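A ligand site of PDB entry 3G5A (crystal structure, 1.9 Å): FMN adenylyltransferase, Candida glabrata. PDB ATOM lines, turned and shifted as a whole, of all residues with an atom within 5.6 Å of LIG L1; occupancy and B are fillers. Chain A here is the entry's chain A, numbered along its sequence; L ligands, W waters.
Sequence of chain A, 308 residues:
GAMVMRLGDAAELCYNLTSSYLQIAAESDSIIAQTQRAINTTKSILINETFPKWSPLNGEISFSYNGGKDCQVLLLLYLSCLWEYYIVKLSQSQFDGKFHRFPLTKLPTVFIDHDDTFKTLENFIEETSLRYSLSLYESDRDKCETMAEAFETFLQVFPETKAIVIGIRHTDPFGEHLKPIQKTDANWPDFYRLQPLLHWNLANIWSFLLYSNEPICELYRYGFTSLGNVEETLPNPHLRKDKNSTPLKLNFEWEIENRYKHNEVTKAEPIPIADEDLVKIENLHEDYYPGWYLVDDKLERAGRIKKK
O of Phe 191 is in hydrogen-bond range of N of Thr 184, 3.0 Å away. The backbone carbonyl oxygen of Lys 183 lies within hydrogen-bond range of the guanidinium group of Arg 193 (2.9 Å). The side-chain carboxylate (OD1) of Asp 185 is in salt-bridge range of the guanidinium group (NH2) of Arg 193, 3.7 Å away.
Water W2 bridges NE1 of Trp 188 (2.8 Å) and O5 of LIG L1 (2.9 Å). Water W3 bridges ND2 of Asn 187 (3.0 Å) and O1 of LIG L1 (3.0 Å).
A nitrogen (N2) of LIG L1 sits close to the guanidinium group (NH1) of Arg 193, 3.5 Å away. Residues that only touch LIG L1: Thr 146 (3.5 Å), Phe 151 (3.6 Å), Ile 164 (3.7 Å), Ile 166 (3.4 Å), Thr 184 (3.3 Å), Trp 188 (3.2 Å) and Phe 191 (3.8 Å). Hydrophobic or aromatic side chains that line LIG L1: Met 147, Phe 151, Ile 164, Ile 166, Trp 188 and Phe 191. The nearest printed residue that does not touch LIG L1 is Ser 64 (4.1 Å).
OG of Ser 64 is in hydrogen-bond range of O12 of LG2 L2. The backbone carbonyl oxygen (O) of Ser 64 is in hydrogen-bond range of an oxygen (O12) of LG2 L2 (3.0 Å). An oxygen (O2) of LIG L1 lies within hydrogen-bond range of the backbone NH of Asp 185 (2.9 Å). An oxygen (O9) of LIG L1 sits at hydrogen-bond distance from the backbone NH of Met 147 (2.7 Å). A nitrogen (N2) of LIG L1 is in hydrogen-bond range of the side-chain carboxylate of Asp 185, 2.7 Å away.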
ATOM      1  N   SER A  64      16.132   6.178 -19.290  1.00  0.00           N
ATOM      2  CA  SER A  64      16.804   6.981 -18.237  1.00  0.00           C
ATOM      3  C   SER A  64      16.725   8.496 -18.557  1.00  0.00           C
ATOM      4  O   SER A  64      17.201   8.972 -19.589  1.00  0.00           O
ATOM      5  CB  SER A  64      18.235   6.497 -17.954  1.00  0.00           C
ATOM      6  OG  SER A  64      19.110   6.837 -19.004  1.00  0.00           O
ATOM      7  N   GLU A 145      23.665   6.600  -1.827  1.00  0.00           N
ATOM      8  CA  GLU A 145      23.950   5.366  -2.556  1.00  0.00           C
ATOM      9  C   GLU A 145      24.580   5.714  -3.909  1.00  0.00           C
ATOM     10  O   GLU A 145      24.459   6.845  -4.388  1.00  0.00           O
ATOM     11  CB  GLU A 145      22.642   4.565  -2.720  1.00  0.00           C
ATOM     12  CG  GLU A 145      21.623   5.190  -3.662  1.00  0.00           C
ATOM     13  CD  GLU A 145      20.322   4.430  -3.658  1.00  0.00           C
ATOM     14  OE1 GLU A 145      20.313   3.288  -3.143  1.00  0.00           O
ATOM     15  OE2 GLU A 145      19.295   4.970  -4.158  1.00  0.00           O
ATOM     16  N   THR A 146      25.289   4.764  -4.518  1.00  0.00           N
ATOM     17  CA  THR A 146      25.825   5.015  -5.861  1.00  0.00           C
ATOM     18  C   THR A 146      24.697   4.871  -6.911  1.00  0.00           C
ATOM     19  O   THR A 146      23.608   4.342  -6.607  1.00  0.00           O
ATOM     20  CB  THR A 146      26.980   4.043  -6.223  1.00  0.00           C
ATOM     21  OG1 THR A 146      26.470   2.709  -6.215  1.00  0.00           O
ATOM     22  CG2 THR A 146      28.139   4.148  -5.194  1.00  0.00           C
ATOM     23  N   MET A 147      24.952   5.348  -8.127  1.00  0.00           N
ATOM     24  CA  MET A 147      23.989   5.129  -9.240  1.00  0.00           C
ATOM     25  C   MET A 147      23.698   3.649  -9.490  1.00  0.00           C
ATOM     26  O   MET A 147      22.547   3.268  -9.696  1.00  0.00           O
ATOM     27  CB  MET A 147      24.507   5.774 -10.527  1.00  0.00           C
ATOM     28  CG  MET A 147      24.514   7.287 -10.443  1.00  0.00           C
ATOM     29  SD  MET A 147      22.866   7.893 -10.700  1.00  0.00           S
ATOM     30  CE  MET A 147      22.874   7.818 -12.517  1.00  0.00           C
ATOM     31  N   ALA A 148      24.748   2.848  -9.475  1.00  0.00           N
ATOM     32  CA  ALA A 148      24.654   1.376  -9.559  1.00  0.00           C
ATOM     33  C   ALA A 148      23.686   0.810  -8.535  1.00  0.00           C
ATOM     34  O   ALA A 148      22.826  -0.039  -8.860  1.00  0.00           O
ATOM     35  CB  ALA A 148      26.035   0.740  -9.371  1.00  0.00           C
ATOM     36  N   PHE A 151      20.126   1.794  -9.257  1.00  0.00           N
ATOM     37  CA  PHE A 151      19.613   0.998 -10.382  1.00  0.00           C
ATOM     38  C   PHE A 151      19.374  -0.471 -10.008  1.00  0.00           C
ATOM     39  O   PHE A 151      18.486  -1.113 -10.579  1.00  0.00           O
ATOM     40  CB  PHE A 151      20.482   1.143 -11.642  1.00  0.00           C
ATOM     41  CG  PHE A 151      20.104   2.345 -12.502  1.00  0.00           C
ATOM     42  CD1 PHE A 151      18.996   2.284 -13.371  1.00  0.00           C
ATOM     43  CD2 PHE A 151      20.826   3.518 -12.417  1.00  0.00           C
ATOM     44  CE1 PHE A 151      18.634   3.390 -14.130  1.00  0.00           C
ATOM     45  CE2 PHE A 151      20.475   4.643 -13.180  1.00  0.00           C
ATOM     46  CZ  PHE A 151      19.362   4.580 -14.028  1.00  0.00           C
ATOM     47  N   ILE A 164      18.088  -0.354 -20.855  1.00  0.00           N
ATOM     48  CA  ILE A 164      17.824   1.023 -20.426  1.00  0.00           C
ATOM     49  C   ILE A 164      18.472   2.025 -21.382  1.00  0.00           C
ATOM     50  O   ILE A 164      19.663   1.942 -21.669  1.00  0.00           O
ATOM     51  CB  ILE A 164      18.258   1.272 -18.950  1.00  0.00           C
ATOM     52  CG1 ILE A 164      17.525   0.322 -18.004  1.00  0.00           C
ATOM     53  CG2 ILE A 164      18.048   2.755 -18.523  1.00  0.00           C
ATOM     54  CD1 ILE A 164      17.959   0.441 -16.522  1.00  0.00           C
ATOM     55  N   ILE A 166      19.975   5.495 -22.577  1.00  0.00           N
ATOM     56  CA  ILE A 166      20.848   6.484 -21.914  1.00  0.00           C
ATOM     57  C   ILE A 166      21.352   7.513 -22.939  1.00  0.00           C
ATOM     58  O   ILE A 166      21.826   7.133 -24.016  1.00  0.00           O
ATOM     59  CB  ILE A 166      22.094   5.812 -21.275  1.00  0.00           C
ATOM     60  CG1 ILE A 166      21.695   4.624 -20.423  1.00  0.00           C
ATOM     61  CG2 ILE A 166      22.960   6.845 -20.451  1.00  0.00           C
ATOM     62  CD1 ILE A 166      22.828   3.641 -20.216  1.00  0.00           C
ATOM     63  N   PHE A 174      34.258   9.285 -20.098  1.00  0.00           N
ATOM     64  CA  PHE A 174      34.173   7.829 -20.247  1.00  0.00           C
ATOM     65  C   PHE A 174      33.321   7.409 -21.468  1.00  0.00           C
ATOM     66  O   PHE A 174      32.854   6.256 -21.552  1.00  0.00           O
ATOM     67  CB  PHE A 174      33.723   7.157 -18.948  1.00  0.00           C
ATOM     68  CG  PHE A 174      34.350   7.767 -17.708  1.00  0.00           C
ATOM     69  CD1 PHE A 174      35.672   7.474 -17.378  1.00  0.00           C
ATOM     70  CD2 PHE A 174      33.611   8.616 -16.865  1.00  0.00           C
ATOM     71  CE1 PHE A 174      36.259   8.033 -16.226  1.00  0.00           C
ATOM     72  CE2 PHE A 174      34.186   9.203 -15.736  1.00  0.00           C
ATOM     73  CZ  PHE A 174      35.508   8.910 -15.405  1.00  0.00           C
ATOM     74  N   LYS A 183      26.249  -4.500 -22.676  1.00  0.00           N
ATOM     75  CA  LYS A 183      25.895  -4.825 -21.286  1.00  0.00           C
ATOM     76  C   LYS A 183      26.612  -3.840 -20.357  1.00  0.00           C
ATOM     77  O   LYS A 183      27.656  -3.293 -20.695  1.00  0.00           O
ATOM     78  CB  LYS A 183      26.278  -6.276 -20.950  1.00  0.00           C
ATOM     79  CG  LYS A 183      25.381  -7.328 -21.621  1.00  0.00           C
ATOM     80  CD  LYS A 183      25.841  -8.753 -21.303  1.00  0.00           C
ATOM     81  CE  LYS A 183      24.820  -9.811 -21.725  1.00  0.00           C
ATOM     82  NZ  LYS A 183      23.572  -9.773 -20.898  1.00  0.00           N
ATOM     83  N   THR A 184      26.010  -3.625 -19.193  1.00  0.00           N
ATOM     84  CA  THR A 184      26.622  -2.896 -18.088  1.00  0.00           C
ATOM     85  C   THR A 184      27.862  -3.655 -17.632  1.00  0.00           C
ATOM     86  O   THR A 184      28.030  -4.843 -17.965  1.00  0.00           O
ATOM     87  CB  THR A 184      25.681  -2.826 -16.904  1.00  0.00           C
ATOM     88  OG1 THR A 184      25.212  -4.168 -16.584  1.00  0.00           O
ATOM     89  CG2 THR A 184      24.491  -1.891 -17.207  1.00  0.00           C
ATOM     90  N   ASP A 185      28.698  -2.986 -16.829  1.00  0.00           N
ATOM     91  CA  ASP A 185      29.886  -3.612 -16.247  1.00  0.00           C
ATOM     92  C   ASP A 185      29.563  -4.513 -15.067  1.00  0.00           C
ATOM     93  O   ASP A 185      28.458  -4.480 -14.533  1.00  0.00           O
ATOM     94  CB  ASP A 185      30.925  -2.554 -15.849  1.00  0.00           C
ATOM     95  CG  ASP A 185      31.403  -1.769 -17.043  1.00  0.00           C
ATOM     96  OD1 ASP A 185      31.708  -2.398 -18.078  1.00  0.00           O
ATOM     97  OD2 ASP A 185      31.443  -0.520 -16.963  1.00  0.00           O
ATOM     98  N   ASN A 187      30.364  -4.447 -11.986  1.00  0.00           N
ATOM     99  CA  ASN A 187      30.020  -3.770 -10.714  1.00  0.00           C
ATOM    100  C   ASN A 187      28.640  -3.097 -10.722  1.00  0.00           C
ATOM    101  O   ASN A 187      28.246  -2.442  -9.736  1.00  0.00           O
ATOM    102  CB  ASN A 187      31.100  -2.721 -10.364  1.00  0.00           C
ATOM    103  CG  ASN A 187      31.198  -1.585 -11.418  1.00  0.00           C
ATOM    104  OD1 ASN A 187      31.184  -1.826 -12.626  1.00  0.00           O
ATOM    105  ND2 ASN A 187      31.310  -0.360 -10.948  1.00  0.00           N
ATOM    106  N   TRP A 188      27.903  -3.265 -11.823  1.00  0.00           N
ATOM    107  CA  TRP A 188      26.543  -2.735 -11.961  1.00  0.00           C
ATOM    108  C   TRP A 188      25.534  -3.866 -11.924  1.00  0.00           C
ATOM    109  O   TRP A 188      25.908  -5.029 -12.115  1.00  0.00           O
ATOM    110  CB  TRP A 188      26.407  -1.975 -13.282  1.00  0.00           C
ATOM    111  CG  TRP A 188      26.759  -0.562 -13.148  1.00  0.00           C
ATOM    112  CD1 TRP A 188      28.013  -0.033 -12.929  1.00  0.00           C
ATOM    113  CD2 TRP A 188      25.858   0.535 -13.218  1.00  0.00           C
ATOM    114  NE1 TRP A 188      27.922   1.334 -12.828  1.00  0.00           N
ATOM    115  CE2 TRP A 188      26.612   1.706 -13.017  1.00  0.00           C
ATOM    116  CE3 TRP A 188      24.475   0.647 -13.432  1.00  0.00           C
ATOM    117  CZ2 TRP A 188      26.031   2.985 -13.007  1.00  0.00           C
ATOM    118  CZ3 TRP A 188      23.903   1.907 -13.432  1.00  0.00           C
ATOM    119  CH2 TRP A 188      24.671   3.052 -13.199  1.00  0.00           C
ATOM    120  N   PHE A 191      22.061  -5.378 -17.055  1.00  0.00           N
ATOM    121  CA  PHE A 191      21.118  -5.037 -18.120  1.00  0.00           C
ATOM    122  C   PHE A 191      21.912  -4.524 -19.330  1.00  0.00           C
ATOM    123  O   PHE A 191      23.137  -4.322 -19.228  1.00  0.00           O
ATOM    124  CB  PHE A 191      20.012  -4.032 -17.637  1.00  0.00           C
ATOM    125  CG  PHE A 191      20.551  -2.723 -17.053  1.00  0.00           C
ATOM    126  CD1 PHE A 191      20.714  -2.564 -15.669  1.00  0.00           C
ATOM    127  CD2 PHE A 191      20.850  -1.635 -17.883  1.00  0.00           C
ATOM    128  CE1 PHE A 191      21.222  -1.322 -15.132  1.00  0.00           C
ATOM    129  CE2 PHE A 191      21.346  -0.437 -17.359  1.00  0.00           C
ATOM    130  CZ  PHE A 191      21.522  -0.281 -15.977  1.00  0.00           C
ATOM    131  N   ARG A 193      22.735  -1.495 -21.745  1.00  0.00           N
ATOM    132  CA  ARG A 193      22.747  -0.076 -21.998  1.00  0.00           C
ATOM    133  C   ARG A 193      22.457   0.170 -23.482  1.00  0.00           C
ATOM    134  O   ARG A 193      23.094  -0.425 -24.378  1.00  0.00           O
ATOM    135  CB  ARG A 193      24.125   0.486 -21.694  1.00  0.00           C
ATOM    136  CG  ARG A 193      24.580   0.321 -20.262  1.00  0.00           C
ATOM    137  CD  ARG A 193      25.934   1.009 -20.154  1.00  0.00           C
ATOM    138  NE  ARG A 193      26.979   0.015 -20.298  1.00  0.00           N
ATOM    139  CZ  ARG A 193      28.263   0.220 -20.013  1.00  0.00           C
ATOM    140  NH1 ARG A 193      28.693   1.423 -19.590  1.00  0.00           N
ATOM    141  NH2 ARG A 193      29.119  -0.800 -20.108  1.00  0.00           N
HETATM  142  N1  LIG L   1      29.085   3.474 -15.903  1.00  0.00           N
HETATM  143  C1  LIG L   1      29.994   2.428 -15.953  1.00  0.00           C
HETATM  144  O1  LIG L   1      31.217   2.605 -15.735  1.00  0.00           O
HETATM  145  N2  LIG L   1      29.498   1.160 -16.232  1.00  0.00           N
HETATM  146  C2  LIG L   1      28.168   0.926 -16.443  1.00  0.00           C
HETATM  147  O2  LIG L   1      27.799  -0.248 -16.574  1.00  0.00           O
HETATM  148  C3  LIG L   1      27.267   1.988 -16.417  1.00  0.00           C
HETATM  149  N3  LIG L   1      25.923   1.780 -16.660  1.00  0.00           N
HETATM  150  C4  LIG L   1      25.029   2.871 -16.628  1.00  0.00           C
HETATM  151  C5  LIG L   1      23.659   2.682 -16.878  1.00  0.00           C
HETATM  152  C6  LIG L   1      22.749   3.751 -16.821  1.00  0.00           C
HETATM  153  C7  LIG L   1      21.281   3.453 -16.834  1.00  0.00           C
HETATM  154  C8  LIG L   1      23.237   5.049 -16.544  1.00  0.00           C
HETATM  155  C9  LIG L   1      22.342   6.269 -16.528  1.00  0.00           C
HETATM  156  C10 LIG L   1      24.598   5.244 -16.313  1.00  0.00           C
HETATM  157  C11 LIG L   1      25.506   4.163 -16.359  1.00  0.00           C
HETATM  158  N4  LIG L   1      26.865   4.379 -16.130  1.00  0.00           N
HETATM  159  C12 LIG L   1      27.739   3.288 -16.148  1.00  0.00           C
HETATM  160  C13 LIG L   1      27.368   5.806 -15.944  1.00  0.00           C
HETATM  161  C14 LIG L   1      27.687   6.100 -14.473  1.00  0.00           C
HETATM  162  O3  LIG L   1      26.489   6.110 -13.704  1.00  0.00           O
HETATM  163  C15 LIG L   1      28.506   7.373 -14.153  1.00  0.00           C
HETATM  164  O4  LIG L   1      29.633   7.460 -15.002  1.00  0.00           O
HETATM  165  C16 LIG L   1      29.076   7.353 -12.720  1.00  0.00           C
HETATM  166  O5  LIG L   1      29.980   6.282 -12.622  1.00  0.00           O
HETATM  167  C17 LIG L   1      28.058   7.220 -11.577  1.00  0.00           C
HETATM  168  O6  LIG L   1      28.501   7.817 -10.372  1.00  0.00           O
HETATM  169  P1  LIG L   1      28.385   7.063  -8.932  1.00  0.00           P
HETATM  170  O7  LIG L   1      29.316   7.734  -7.952  1.00  0.00           O
HETATM  171  O8  LIG L   1      28.857   5.643  -9.098  1.00  0.00           O
HETATM  172  O9  LIG L   1      27.001   7.059  -8.393  1.00  0.00           O
HETATM  173  P1  LG2 L   2      23.793  17.825 -19.719  1.00  0.00           P
HETATM  174  O1  LG2 L   2      23.912  17.648 -18.212  1.00  0.00           O
HETATM  175  O2  LG2 L   2      23.498  19.236 -20.139  1.00  0.00           O
HETATM  176  O3  LG2 L   2      24.979  17.274 -20.458  1.00  0.00           O
HETATM  177  P2  LG2 L   2      22.153  15.387 -20.065  1.00  0.00           P
HETATM  178  O4  LG2 L   2      20.807  15.034 -20.616  1.00  0.00           O
HETATM  179  O5  LG2 L   2      23.346  14.627 -20.595  1.00  0.00           O
HETATM  180  O6  LG2 L   2      22.458  16.969 -20.199  1.00  0.00           O
HETATM  181  P3  LG2 L   2      23.497  14.028 -17.573  1.00  0.00           P
HETATM  182  O7  LG2 L   2      23.339  14.054 -16.070  1.00  0.00           O
HETATM  183  O8  LG2 L   2      24.773  14.651 -18.088  1.00  0.00           O
HETATM  184  C1  LG2 L   2      22.094  14.955 -18.286  1.00  0.00           C
HETATM  185  O9  LG2 L   2      23.525  12.430 -18.002  1.00  0.00           O
HETATM  186  C2  LG2 L   2      23.824  11.783 -19.280  1.00  0.00           C
HETATM  187  C3  LG2 L   2      22.876  10.605 -19.628  1.00  0.00           C
HETATM  188  O10 LG2 L   2      22.852   9.706 -18.505  1.00  0.00           O
HETATM  189  C4  LG2 L   2      21.503  11.283 -19.598  1.00  0.00           C
HETATM  190  O11 LG2 L   2      21.035  11.665 -20.880  1.00  0.00           O
HETATM  191  C5  LG2 L   2      20.589  10.263 -18.947  1.00  0.00           C
HETATM  192  O12 LG2 L   2      20.121   9.306 -19.927  1.00  0.00           O
HETATM  193  C6  LG2 L   2      21.527   9.503 -18.034  1.00  0.00           C
HETATM  194  N1  LG2 L   2      21.487  10.006 -16.634  1.00  0.00           N
HETATM  195  C7  LG2 L   2      22.463  10.717 -16.026  1.00  0.00           C
HETATM  196  N2  LG2 L   2      22.096  10.988 -14.760  1.00  0.00           N
HETATM  197  C8  LG2 L   2      20.886  10.417 -14.551  1.00  0.00           C
HETATM  198  C9  LG2 L   2      20.004  10.393 -13.459  1.00  0.00           C
HETATM  199  N3  LG2 L   2      20.295  10.977 -12.264  1.00  0.00           N
HETATM  200  N4  LG2 L   2      18.828   9.736 -13.604  1.00  0.00           N
HETATM  201  C10 LG2 L   2      18.473   9.134 -14.763  1.00  0.00           C
HETATM  202  N5  LG2 L   2      19.290   9.177 -15.826  1.00  0.00           N
HETATM  203  C11 LG2 L   2      20.487   9.811 -15.753  1.00  0.00           C
HETATM  204  O   HOH W   1      25.245   8.537 -14.923  1.00  0.00           O
HETATM  205  O   HOH W   2      29.677   3.433 -12.092  1.00  0.00           O
HETATM  206  O   HOH W   3      32.015   1.826 -12.906  1.00  0.00           O
HETATM  207  O   HOH W   4      32.785  -0.125 -14.662  1.00  0.00           O
HETATM  208  O   HOH W   5      28.114   7.850  -4.786  1.00  0.00           O
HETATM  209  O   HOH W   6      29.193   8.234 -17.417  1.00  0.00           O
